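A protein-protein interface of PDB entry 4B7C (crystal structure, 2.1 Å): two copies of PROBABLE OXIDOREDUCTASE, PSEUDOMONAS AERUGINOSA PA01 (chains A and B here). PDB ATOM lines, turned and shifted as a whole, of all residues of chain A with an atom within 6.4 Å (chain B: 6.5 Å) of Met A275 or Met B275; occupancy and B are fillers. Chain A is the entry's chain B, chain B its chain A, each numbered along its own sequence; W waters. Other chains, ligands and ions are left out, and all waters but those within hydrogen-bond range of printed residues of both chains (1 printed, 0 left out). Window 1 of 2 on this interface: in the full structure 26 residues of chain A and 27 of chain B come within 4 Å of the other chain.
Water W1 lies within hydrogen-bond range of OD2 of Asp B224 and OH of Tyr A265.
The backbone carbonyl oxygen of Met B275 is in hydrogen-bond range of the backbone NH of Met A275 (2.7 Å). N of Gly B277 is in hydrogen-bond range of O of Ala A273. The side-chain carboxylate (OE1) of Glu B276 lies within salt-bridge range of the guanidinium group (NE) of Arg A274. NE of Arg B274 is in salt-bridge range of OE1 of Glu A276, 3.2 Å away. N of Gly A277 is in hydrogen-bond range of O of Ala B273 (3.1 Å). NE of Arg A274 sits close to NH1 of Arg B274 (2.9 Å).
Printed residues of chain A that touch a printed residue of chain B: Leu A231, Leu A246, Pro A262, Tyr A265, Leu A268, Ala A273, Arg A274, Met A275, Glu A276 and Gly A277. Hydrophobic or aromatic side chains of chain A within 4 Å of the printed part of chain B: Leu A231, Leu A246, Pro A262, Tyr A265 and Met A275. Among the printed residues, Asp or Glu carboxylates within 4 Å of a Lys or Arg side-chain nitrogen of the other chain: Arg A274 with Glu B276 (3.2 Å) and Glu A276 with Arg B274 (3.2 Å).
The backbone carbonyl oxygen (O) of Glu B276 sits at hydrogen-bond distance from the backbone NH (N) of Leu B246, at 2.8 Å. O of Ile B244 sits at hydrogen-bond distance from N of Glu B276 (2.8 Å). The backbone carbonyl oxygen of Leu A268 sits at hydrogen-bond distance from the backbone NH of Ala A273 (2.8 Å). The backbone carbonyl oxygen (O) of Leu B268 sits at hydrogen-bond distance from the backbone NH (N) of Ala B273 (2.8 Å). The guanidinium group (NH1) of Arg B274 is in salt-bridge range of the side-chain carboxylate (OE1) of Glu B276, at 3.5 Å. The backbone carbonyl oxygen (O) of Ala A242 is in hydrogen-bond range of the backbone NH (N) of Arg A274 (2.9 Å).
Leu A231 touches Tyr B265, and with the chains exchanged Tyr A265 touches Leu B231. Leu A268 touches Gly B277, and with the chains exchanged Gly A277 touches Leu B268. Ala A273 touches Glu B276, and with the chains exchanged Glu A276 touches Ala B273. Ala A273 touches Gly B277, and with the chains exchanged Gly A277 touches Ala B273.
Leu A231 touches Tyr B265. Leu A246 touches Tyr B265. CD of Pro B262 touches O of Pro A262, 3.7 Å away. CD of Pro A262 touches CD1 of Tyr B265, at 3.8 Å. Tyr A265 touches Leu B231 (CE2 to CD2, 3.7 Å). Tyr A265 touches Pro B262. Ala A273 touches Glu B276. Met B275 touches Arg A274 (O to CA, 3.5 Å). Arg B274 touches Met A275. Glu A276 touches Ala B273 (CA to O, 3.5 Å).
Of chain B, only Arg B274 (3.6 Å) and Met B275 (2.7 Å) come within 4 Å of Met A275. Of the printed residues of chain B, Gly A277 touches Leu B268 and Ala B273. Printed residues of chain B within 4 Å of Arg A274: Arg B274 (2.9 Å), Met B275 (3.5 Å) and Glu B276 (3.2 Å). The nearest residue of chain B that does not touch Met A275 is Leu B268 (4.1 Å). The nearest residue of chain A that does not touch Met B275 is Ala A273 (4.1 Å).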
ATOM      1  N   LEU A 231     -15.922   0.292 -16.791  1.00  0.00           N
ATOM      2  CA  LEU A 231     -16.029   1.314 -17.843  1.00  0.00           C
ATOM      3  C   LEU A 231     -14.794   2.215 -17.843  1.00  0.00           C
ATOM      4  O   LEU A 231     -14.193   2.478 -18.889  1.00  0.00           O
ATOM      5  CB  LEU A 231     -17.289   2.165 -17.635  1.00  0.00           C
ATOM      6  CG  LEU A 231     -17.386   3.482 -18.420  1.00  0.00           C
ATOM      7  CD1 LEU A 231     -17.341   3.242 -19.910  1.00  0.00           C
ATOM      8  CD2 LEU A 231     -18.650   4.217 -17.999  1.00  0.00           C
ATOM      9  N   LEU A 235     -12.021   2.596 -20.903  1.00  0.00           N
ATOM     10  CA  LEU A 235     -11.748   3.915 -21.520  1.00  0.00           C
ATOM     11  C   LEU A 235     -10.264   4.163 -21.786  1.00  0.00           C
ATOM     12  O   LEU A 235      -9.913   4.830 -22.753  1.00  0.00           O
ATOM     13  CB  LEU A 235     -12.297   5.046 -20.643  1.00  0.00           C
ATOM     14  CG  LEU A 235     -13.793   5.342 -20.835  1.00  0.00           C
ATOM     15  CD1 LEU A 235     -14.381   6.123 -19.681  1.00  0.00           C
ATOM     16  CD2 LEU A 235     -13.999   6.084 -22.150  1.00  0.00           C
ATOM     17  N   ALA A 242     -13.500   5.305 -31.494  1.00  0.00           N
ATOM     18  CA  ALA A 242     -14.244   4.281 -30.790  1.00  0.00           C
ATOM     19  C   ALA A 242     -15.668   4.738 -30.523  1.00  0.00           C
ATOM     20  O   ALA A 242     -15.940   5.939 -30.406  1.00  0.00           O
ATOM     21  CB  ALA A 242     -13.573   3.958 -29.472  1.00  0.00           C
ATOM     22  N   ARG A 243     -16.561   3.767 -30.394  1.00  0.00           N
ATOM     23  CA  ARG A 243     -17.943   4.018 -29.980  1.00  0.00           C
ATOM     24  C   ARG A 243     -18.220   3.264 -28.707  1.00  0.00           C
ATOM     25  O   ARG A 243     -18.013   2.050 -28.627  1.00  0.00           O
ATOM     26  CB  ARG A 243     -18.934   3.592 -31.053  1.00  0.00           C
ATOM     27  CG  ARG A 243     -18.956   4.505 -32.264  1.00  0.00           C
ATOM     28  CD  ARG A 243     -17.838   4.176 -33.246  1.00  0.00           C
ATOM     29  NE  ARG A 243     -18.012   2.935 -33.941  1.00  0.00           N
ATOM     30  CZ  ARG A 243     -17.034   2.143 -34.369  1.00  0.00           C
ATOM     31  NH1 ARG A 243     -15.727   2.373 -34.165  1.00  0.00           N
ATOM     32  NH2 ARG A 243     -17.409   1.074 -35.016  1.00  0.00           N
ATOM     33  N   ILE A 244     -18.681   3.996 -27.708  1.00  0.00           N
ATOM     34  CA  ILE A 244     -19.124   3.427 -26.454  1.00  0.00           C
ATOM     35  C   ILE A 244     -20.635   3.557 -26.369  1.00  0.00           C
ATOM     36  O   ILE A 244     -21.178   4.670 -26.421  1.00  0.00           O
ATOM     37  CB  ILE A 244     -18.502   4.131 -25.240  1.00  0.00           C
ATOM     38  CG1 ILE A 244     -16.974   3.984 -25.278  1.00  0.00           C
ATOM     39  CG2 ILE A 244     -19.065   3.569 -23.944  1.00  0.00           C
ATOM     40  CD1 ILE A 244     -16.286   4.548 -24.057  1.00  0.00           C
ATOM     41  N   VAL A 245     -21.321   2.421 -26.255  1.00  0.00           N
ATOM     42  CA  VAL A 245     -22.768   2.439 -26.098  1.00  0.00           C
ATOM     43  C   VAL A 245     -23.139   2.098 -24.671  1.00  0.00           C
ATOM     44  O   VAL A 245     -22.733   1.062 -24.133  1.00  0.00           O
ATOM     45  CB  VAL A 245     -23.487   1.525 -27.122  1.00  0.00           C
ATOM     46  CG1 VAL A 245     -22.950   0.117 -27.084  1.00  0.00           C
ATOM     47  CG2 VAL A 245     -24.986   1.541 -26.871  1.00  0.00           C
ATOM     48  N   LEU A 246     -23.896   3.002 -24.052  1.00  0.00           N
ATOM     49  CA  LEU A 246     -24.355   2.833 -22.685  1.00  0.00           C
ATOM     50  C   LEU A 246     -25.788   2.293 -22.675  1.00  0.00           C
ATOM     51  O   LEU A 246     -26.721   2.955 -23.155  1.00  0.00           O
ATOM     52  CB  LEU A 246     -24.327   4.158 -21.918  1.00  0.00           C
ATOM     53  CG  LEU A 246     -23.004   4.912 -21.895  1.00  0.00           C
ATOM     54  CD1 LEU A 246     -23.201   6.205 -21.099  1.00  0.00           C
ATOM     55  CD2 LEU A 246     -21.886   4.054 -21.311  1.00  0.00           C
ATOM     56  N   PRO A 262     -16.782   8.102 -14.628  1.00  0.00           N
ATOM     57  CA  PRO A 262     -15.509   7.742 -15.251  1.00  0.00           C
ATOM     58  C   PRO A 262     -14.464   8.866 -15.270  1.00  0.00           C
ATOM     59  O   PRO A 262     -14.573   9.820 -16.045  1.00  0.00           O
ATOM     60  CB  PRO A 262     -15.913   7.355 -16.673  1.00  0.00           C
ATOM     61  CG  PRO A 262     -17.166   8.100 -16.933  1.00  0.00           C
ATOM     62  CD  PRO A 262     -17.857   8.277 -15.618  1.00  0.00           C
ATOM     63  N   TYR A 265     -12.746   9.814 -18.721  1.00  0.00           N
ATOM     64  CA  TYR A 265     -13.672  10.229 -19.800  1.00  0.00           C
ATOM     65  C   TYR A 265     -12.986  11.059 -20.891  1.00  0.00           C
ATOM     66  O   TYR A 265     -13.409  11.039 -22.038  1.00  0.00           O
ATOM     67  CB  TYR A 265     -14.879  10.986 -19.232  1.00  0.00           C
ATOM     68  CG  TYR A 265     -14.637  12.457 -19.035  1.00  0.00           C
ATOM     69  CD1 TYR A 265     -13.985  12.933 -17.900  1.00  0.00           C
ATOM     70  CD2 TYR A 265     -15.060  13.380 -19.984  1.00  0.00           C
ATOM     71  CE1 TYR A 265     -13.758  14.288 -17.722  1.00  0.00           C
ATOM     72  CE2 TYR A 265     -14.832  14.732 -19.822  1.00  0.00           C
ATOM     73  CZ  TYR A 265     -14.186  15.185 -18.693  1.00  0.00           C
ATOM     74  OH  TYR A 265     -13.961  16.523 -18.550  1.00  0.00           O
ATOM     75  N   LEU A 268     -12.096  10.078 -24.464  1.00  0.00           N
ATOM     76  CA  LEU A 268     -13.009  10.410 -25.592  1.00  0.00           C
ATOM     77  C   LEU A 268     -12.514  11.573 -26.431  1.00  0.00           C
ATOM     78  O   LEU A 268     -12.705  11.605 -27.651  1.00  0.00           O
ATOM     79  CB  LEU A 268     -14.408  10.737 -25.078  1.00  0.00           C
ATOM     80  CG  LEU A 268     -15.182   9.622 -24.380  1.00  0.00           C
ATOM     81  CD1 LEU A 268     -16.458  10.167 -23.753  1.00  0.00           C
ATOM     82  CD2 LEU A 268     -15.465   8.477 -25.340  1.00  0.00           C
ATOM     83  N   ALA A 273     -13.518   9.981 -29.767  1.00  0.00           N
ATOM     84  CA  ALA A 273     -14.449   8.880 -29.662  1.00  0.00           C
ATOM     85  C   ALA A 273     -15.797   9.378 -29.178  1.00  0.00           C
ATOM     86  O   ALA A 273     -15.919  10.501 -28.692  1.00  0.00           O
ATOM     87  CB  ALA A 273     -13.914   7.868 -28.657  1.00  0.00           C
ATOM     88  N   ARG A 274     -16.787   8.492 -29.257  1.00  0.00           N
ATOM     89  CA  ARG A 274     -18.175   8.820 -28.957  1.00  0.00           C
ATOM     90  C   ARG A 274     -18.726   7.916 -27.867  1.00  0.00           C
ATOM     91  O   ARG A 274     -18.531   6.695 -27.894  1.00  0.00           O
ATOM     92  CB  ARG A 274     -19.010   8.684 -30.233  1.00  0.00           C
ATOM     93  CG  ARG A 274     -20.504   8.874 -30.047  1.00  0.00           C
ATOM     94  CD  ARG A 274     -21.265   8.522 -31.313  1.00  0.00           C
ATOM     95  NE  ARG A 274     -20.806   9.310 -32.450  1.00  0.00           N
ATOM     96  CZ  ARG A 274     -20.420   8.826 -33.633  1.00  0.00           C
ATOM     97  NH1 ARG A 274     -20.441   7.523 -33.892  1.00  0.00           N
ATOM     98  NH2 ARG A 274     -20.024   9.670 -34.584  1.00  0.00           N
ATOM     99  N   MET A 275     -19.407   8.526 -26.907  1.00  0.00           N
ATOM    100  CA  MET A 275     -20.116   7.804 -25.871  1.00  0.00           C
ATOM    101  C   MET A 275     -21.589   8.191 -25.948  1.00  0.00           C
ATOM    102  O   MET A 275     -21.945   9.364 -25.815  1.00  0.00           O
ATOM    103  CB  MET A 275     -19.567   8.111 -24.478  1.00  0.00           C
ATOM    104  CG  MET A 275     -20.263   7.363 -23.349  1.00  0.00           C
ATOM    105  SD  MET A 275     -19.647   7.770 -21.704  1.00  0.00           S
ATOM    106  CE  MET A 275     -18.214   6.732 -21.725  1.00  0.00           C
ATOM    107  N   GLU A 276     -22.445   7.185 -26.113  1.00  0.00           N
ATOM    108  CA  GLU A 276     -23.859   7.424 -26.374  1.00  0.00           C
ATOM    109  C   GLU A 276     -24.789   6.455 -25.660  1.00  0.00           C
ATOM    110  O   GLU A 276     -24.563   5.243 -25.638  1.00  0.00           O
ATOM    111  CB  GLU A 276     -24.120   7.385 -27.877  1.00  0.00           C
ATOM    112  CG  GLU A 276     -25.529   7.791 -28.265  1.00  0.00           C
ATOM    113  CD  GLU A 276     -25.709   7.957 -29.765  1.00  0.00           C
ATOM    114  OE1 GLU A 276     -24.710   8.051 -30.499  1.00  0.00           O
ATOM    115  OE2 GLU A 276     -26.868   8.015 -30.205  1.00  0.00           O
ATOM    116  N   GLY A 277     -25.846   7.012 -25.084  1.00  0.00           N
ATOM    117  CA  GLY A 277     -26.857   6.226 -24.405  1.00  0.00           C
ATOM    118  C   GLY A 277     -27.994   5.826 -25.330  1.00  0.00           C
ATOM    119  O   GLY A 277     -28.266   6.499 -26.325  1.00  0.00           O
ATOM    120  N   ASP B 224     -18.167  21.995 -24.451  1.00  0.00           N
ATOM    121  CA  ASP B 224     -17.383  21.920 -23.208  1.00  0.00           C
ATOM    122  C   ASP B 224     -15.889  22.165 -23.410  1.00  0.00           C
ATOM    123  O   ASP B 224     -15.196  21.413 -24.106  1.00  0.00           O
ATOM    124  CB  ASP B 224     -17.578  20.585 -22.510  1.00  0.00           C
ATOM    125  CG  ASP B 224     -17.030  20.584 -21.073  1.00  0.00           C
ATOM    126  OD1 ASP B 224     -16.802  21.679 -20.491  1.00  0.00           O
ATOM    127  OD2 ASP B 224     -16.828  19.478 -20.535  1.00  0.00           O
ATOM    128  N   LEU B 231     -19.302  20.553 -16.178  1.00  0.00           N
ATOM    129  CA  LEU B 231     -19.815  19.488 -17.055  1.00  0.00           C
ATOM    130  C   LEU B 231     -20.835  18.618 -16.330  1.00  0.00           C
ATOM    131  O   LEU B 231     -21.931  18.349 -16.836  1.00  0.00           O
ATOM    132  CB  LEU B 231     -18.675  18.619 -17.582  1.00  0.00           C
ATOM    133  CG  LEU B 231     -19.075  17.281 -18.224  1.00  0.00           C
ATOM    134  CD1 LEU B 231     -20.017  17.501 -19.405  1.00  0.00           C
ATOM    135  CD2 LEU B 231     -17.853  16.470 -18.638  1.00  0.00           C
ATOM    136  N   LEU B 235     -24.867  18.213 -17.288  1.00  0.00           N
ATOM    137  CA  LEU B 235     -25.451  16.890 -17.563  1.00  0.00           C
ATOM    138  C   LEU B 235     -26.828  16.661 -16.931  1.00  0.00           C
ATOM    139  O   LEU B 235     -27.664  15.982 -17.515  1.00  0.00           O
ATOM    140  CB  LEU B 235     -24.512  15.777 -17.115  1.00  0.00           C
ATOM    141  CG  LEU B 235     -23.425  15.442 -18.112  1.00  0.00           C
ATOM    142  CD1 LEU B 235     -22.366  14.618 -17.402  1.00  0.00           C
ATOM    143  CD2 LEU B 235     -23.995  14.672 -19.293  1.00  0.00           C
ATOM    144  N   ALA B 242     -29.557  15.232 -26.770  1.00  0.00           N
ATOM    145  CA  ALA B 242     -28.530  16.255 -26.624  1.00  0.00           C
ATOM    146  C   ALA B 242     -27.190  15.783 -27.161  1.00  0.00           C
ATOM    147  O   ALA B 242     -26.908  14.579 -27.203  1.00  0.00           O
ATOM    148  CB  ALA B 242     -28.388  16.659 -25.158  1.00  0.00           C
ATOM    149  N   ARG B 243     -26.377  16.739 -27.605  1.00  0.00           N
ATOM    150  CA  ARG B 243     -25.014  16.481 -28.030  1.00  0.00           C
ATOM    151  C   ARG B 243     -24.072  17.276 -27.147  1.00  0.00           C
ATOM    152  O   ARG B 243     -24.205  18.502 -27.012  1.00  0.00           O
ATOM    153  CB  ARG B 243     -24.780  16.876 -29.480  1.00  0.00           C
ATOM    154  CG  ARG B 243     -25.428  15.919 -30.476  1.00  0.00           C
ATOM    155  CD  ARG B 243     -26.901  16.226 -30.679  1.00  0.00           C
ATOM    156  NE  ARG B 243     -27.154  17.451 -31.347  1.00  0.00           N
ATOM    157  CZ  ARG B 243     -28.232  18.224 -31.196  1.00  0.00           C
ATOM    158  NH1 ARG B 243     -29.296  18.042 -30.372  1.00  0.00           N
ATOM    159  NH2 ARG B 243     -28.185  19.258 -31.953  1.00  0.00           N
ATOM    160  N   ILE B 244     -23.123  16.569 -26.559  1.00  0.00           N
ATOM    161  CA  ILE B 244     -22.062  17.184 -25.782  1.00  0.00           C
ATOM    162  C   ILE B 244     -20.765  17.039 -26.559  1.00  0.00           C
ATOM    163  O   ILE B 244     -20.359  15.907 -26.874  1.00  0.00           O
ATOM    164  CB  ILE B 244     -21.896  16.523 -24.407  1.00  0.00           C
ATOM    165  CG1 ILE B 244     -23.197  16.697 -23.606  1.00  0.00           C
ATOM    166  CG2 ILE B 244     -20.670  17.109 -23.699  1.00  0.00           C
ATOM    167  CD1 ILE B 244     -23.152  16.176 -22.190  1.00  0.00           C
ATOM    168  N   VAL B 245     -20.146  18.170 -26.905  1.00  0.00           N
ATOM    169  CA  VAL B 245     -18.852  18.151 -27.615  1.00  0.00           C
ATOM    170  C   VAL B 245     -17.744  18.526 -26.637  1.00  0.00           C
ATOM    171  O   VAL B 245     -17.784  19.577 -25.993  1.00  0.00           O
ATOM    172  CB  VAL B 245     -18.798  18.998 -28.927  1.00  0.00           C
ATOM    173  CG1 VAL B 245     -17.537  18.658 -29.700  1.00  0.00           C
ATOM    174  CG2 VAL B 245     -20.039  18.726 -29.758  1.00  0.00           C
ATOM    175  N   LEU B 246     -16.790  17.613 -26.494  1.00  0.00           N
ATOM    176  CA  LEU B 246     -15.637  17.813 -25.619  1.00  0.00           C
ATOM    177  C   LEU B 246     -14.465  18.344 -26.426  1.00  0.00           C
ATOM    178  O   LEU B 246     -13.971  17.674 -27.336  1.00  0.00           O
ATOM    179  CB  LEU B 246     -15.231  16.510 -24.933  1.00  0.00           C
ATOM    180  CG  LEU B 246     -16.291  15.745 -24.151  1.00  0.00           C
ATOM    181  CD1 LEU B 246     -15.736  14.403 -23.686  1.00  0.00           C
ATOM    182  CD2 LEU B 246     -16.829  16.550 -22.994  1.00  0.00           C
ATOM    183  N   PRO B 262     -17.454  12.716 -14.446  1.00  0.00           N
ATOM    184  CA  PRO B 262     -18.850  13.140 -14.293  1.00  0.00           C
ATOM    185  C   PRO B 262     -19.745  12.059 -13.701  1.00  0.00           C
ATOM    186  O   PRO B 262     -20.071  11.076 -14.370  1.00  0.00           O
ATOM    187  CB  PRO B 262     -19.276  13.482 -15.724  1.00  0.00           C
ATOM    188  CG  PRO B 262     -18.381  12.692 -16.599  1.00  0.00           C
ATOM    189  CD  PRO B 262     -17.085  12.515 -15.859  1.00  0.00           C
ATOM    190  N   TYR B 265     -23.076  11.054 -15.580  1.00  0.00           N
ATOM    191  CA  TYR B 265     -22.903  10.602 -16.963  1.00  0.00           C
ATOM    192  C   TYR B 265     -24.087   9.761 -17.471  1.00  0.00           C
ATOM    193  O   TYR B 265     -24.359   9.723 -18.668  1.00  0.00           O
ATOM    194  CB  TYR B 265     -21.592   9.833 -17.142  1.00  0.00           C
ATOM    195  CG  TYR B 265     -21.679   8.376 -16.792  1.00  0.00           C
ATOM    196  CD1 TYR B 265     -21.601   7.949 -15.475  1.00  0.00           C
ATOM    197  CD2 TYR B 265     -21.834   7.419 -17.784  1.00  0.00           C
ATOM    198  CE1 TYR B 265     -21.686   6.598 -15.156  1.00  0.00           C
ATOM    199  CE2 TYR B 265     -21.920   6.072 -17.477  1.00  0.00           C
ATOM    200  CZ  TYR B 265     -21.843   5.670 -16.167  1.00  0.00           C
ATOM    201  OH  TYR B 265     -21.948   4.332 -15.880  1.00  0.00           O
ATOM    202  N   LEU B 268     -26.808  10.654 -19.994  1.00  0.00           N
ATOM    203  CA  LEU B 268     -26.675  10.289 -21.402  1.00  0.00           C
ATOM    204  C   LEU B 268     -27.593   9.119 -21.792  1.00  0.00           C
ATOM    205  O   LEU B 268     -28.064   9.037 -22.928  1.00  0.00           O
ATOM    206  CB  LEU B 268     -25.225   9.924 -21.750  1.00  0.00           C
ATOM    207  CG  LEU B 268     -24.174  11.039 -21.675  1.00  0.00           C
ATOM    208  CD1 LEU B 268     -22.805  10.442 -21.998  1.00  0.00           C
ATOM    209  CD2 LEU B 268     -24.476  12.154 -22.669  1.00  0.00           C
ATOM    210  N   ALA B 273     -28.571  10.591 -25.187  1.00  0.00           N
ATOM    211  CA  ALA B 273     -27.755  11.679 -25.657  1.00  0.00           C
ATOM    212  C   ALA B 273     -26.350  11.187 -25.973  1.00  0.00           C
ATOM    213  O   ALA B 273     -25.970  10.073 -25.609  1.00  0.00           O
ATOM    214  CB  ALA B 273     -27.717  12.763 -24.580  1.00  0.00           C
ATOM    215  N   ARG B 274     -25.578  12.045 -26.630  1.00  0.00           N
ATOM    216  CA  ARG B 274     -24.258  11.708 -27.153  1.00  0.00           C
ATOM    217  C   ARG B 274     -23.185  12.648 -26.580  1.00  0.00           C
ATOM    218  O   ARG B 274     -23.363  13.866 -26.534  1.00  0.00           O
ATOM    219  CB  ARG B 274     -24.276  11.799 -28.673  1.00  0.00           C
ATOM    220  CG  ARG B 274     -22.943  11.575 -29.362  1.00  0.00           C
ATOM    221  CD  ARG B 274     -23.013  11.833 -30.874  1.00  0.00           C
ATOM    222  NE  ARG B 274     -23.773  10.849 -31.674  1.00  0.00           N
ATOM    223  CZ  ARG B 274     -23.563  10.588 -32.982  1.00  0.00           C
ATOM    224  NH1 ARG B 274     -22.635  11.227 -33.717  1.00  0.00           N
ATOM    225  NH2 ARG B 274     -24.296   9.653 -33.577  1.00  0.00           N
ATOM    226  N   MET B 275     -22.074  12.057 -26.142  1.00  0.00           N
ATOM    227  CA  MET B 275     -20.891  12.803 -25.704  1.00  0.00           C
ATOM    228  C   MET B 275     -19.711  12.398 -26.569  1.00  0.00           C
ATOM    229  O   MET B 275     -19.363  11.225 -26.657  1.00  0.00           O
ATOM    230  CB  MET B 275     -20.581  12.546 -24.235  1.00  0.00           C
ATOM    231  CG  MET B 275     -19.379  13.330 -23.722  1.00  0.00           C
ATOM    232  SD  MET B 275     -18.952  12.936 -22.018  1.00  0.00           S
ATOM    233  CE  MET B 275     -20.011  14.048 -21.132  1.00  0.00           C
ATOM    234  N   GLU B 276     -19.118  13.378 -27.232  1.00  0.00           N
ATOM    235  CA  GLU B 276     -18.109  13.114 -28.247  1.00  0.00           C
ATOM    236  C   GLU B 276     -16.944  14.100 -28.212  1.00  0.00           C
ATOM    237  O   GLU B 276     -17.124  15.318 -28.104  1.00  0.00           O
ATOM    238  CB  GLU B 276     -18.738  13.113 -29.637  1.00  0.00           C
ATOM    239  CG  GLU B 276     -17.788  12.686 -30.742  1.00  0.00           C
ATOM    240  CD  GLU B 276     -18.478  12.456 -32.073  1.00  0.00           C
ATOM    241  OE1 GLU B 276     -19.715  12.338 -32.114  1.00  0.00           O
ATOM    242  OE2 GLU B 276     -17.776  12.394 -33.097  1.00  0.00           O
ATOM    243  N   GLY B 277     -15.736  13.558 -28.333  1.00  0.00           N
ATOM    244  CA  GLY B 277     -14.523  14.370 -28.363  1.00  0.00           C
ATOM    245  C   GLY B 277     -14.109  14.739 -29.760  1.00  0.00           C
ATOM    246  O   GLY B 277     -14.447  14.056 -30.735  1.00  0.00           O
HETATM  247  O   HOH W   1     -14.587  18.157 -20.772  1.00  0.00           O
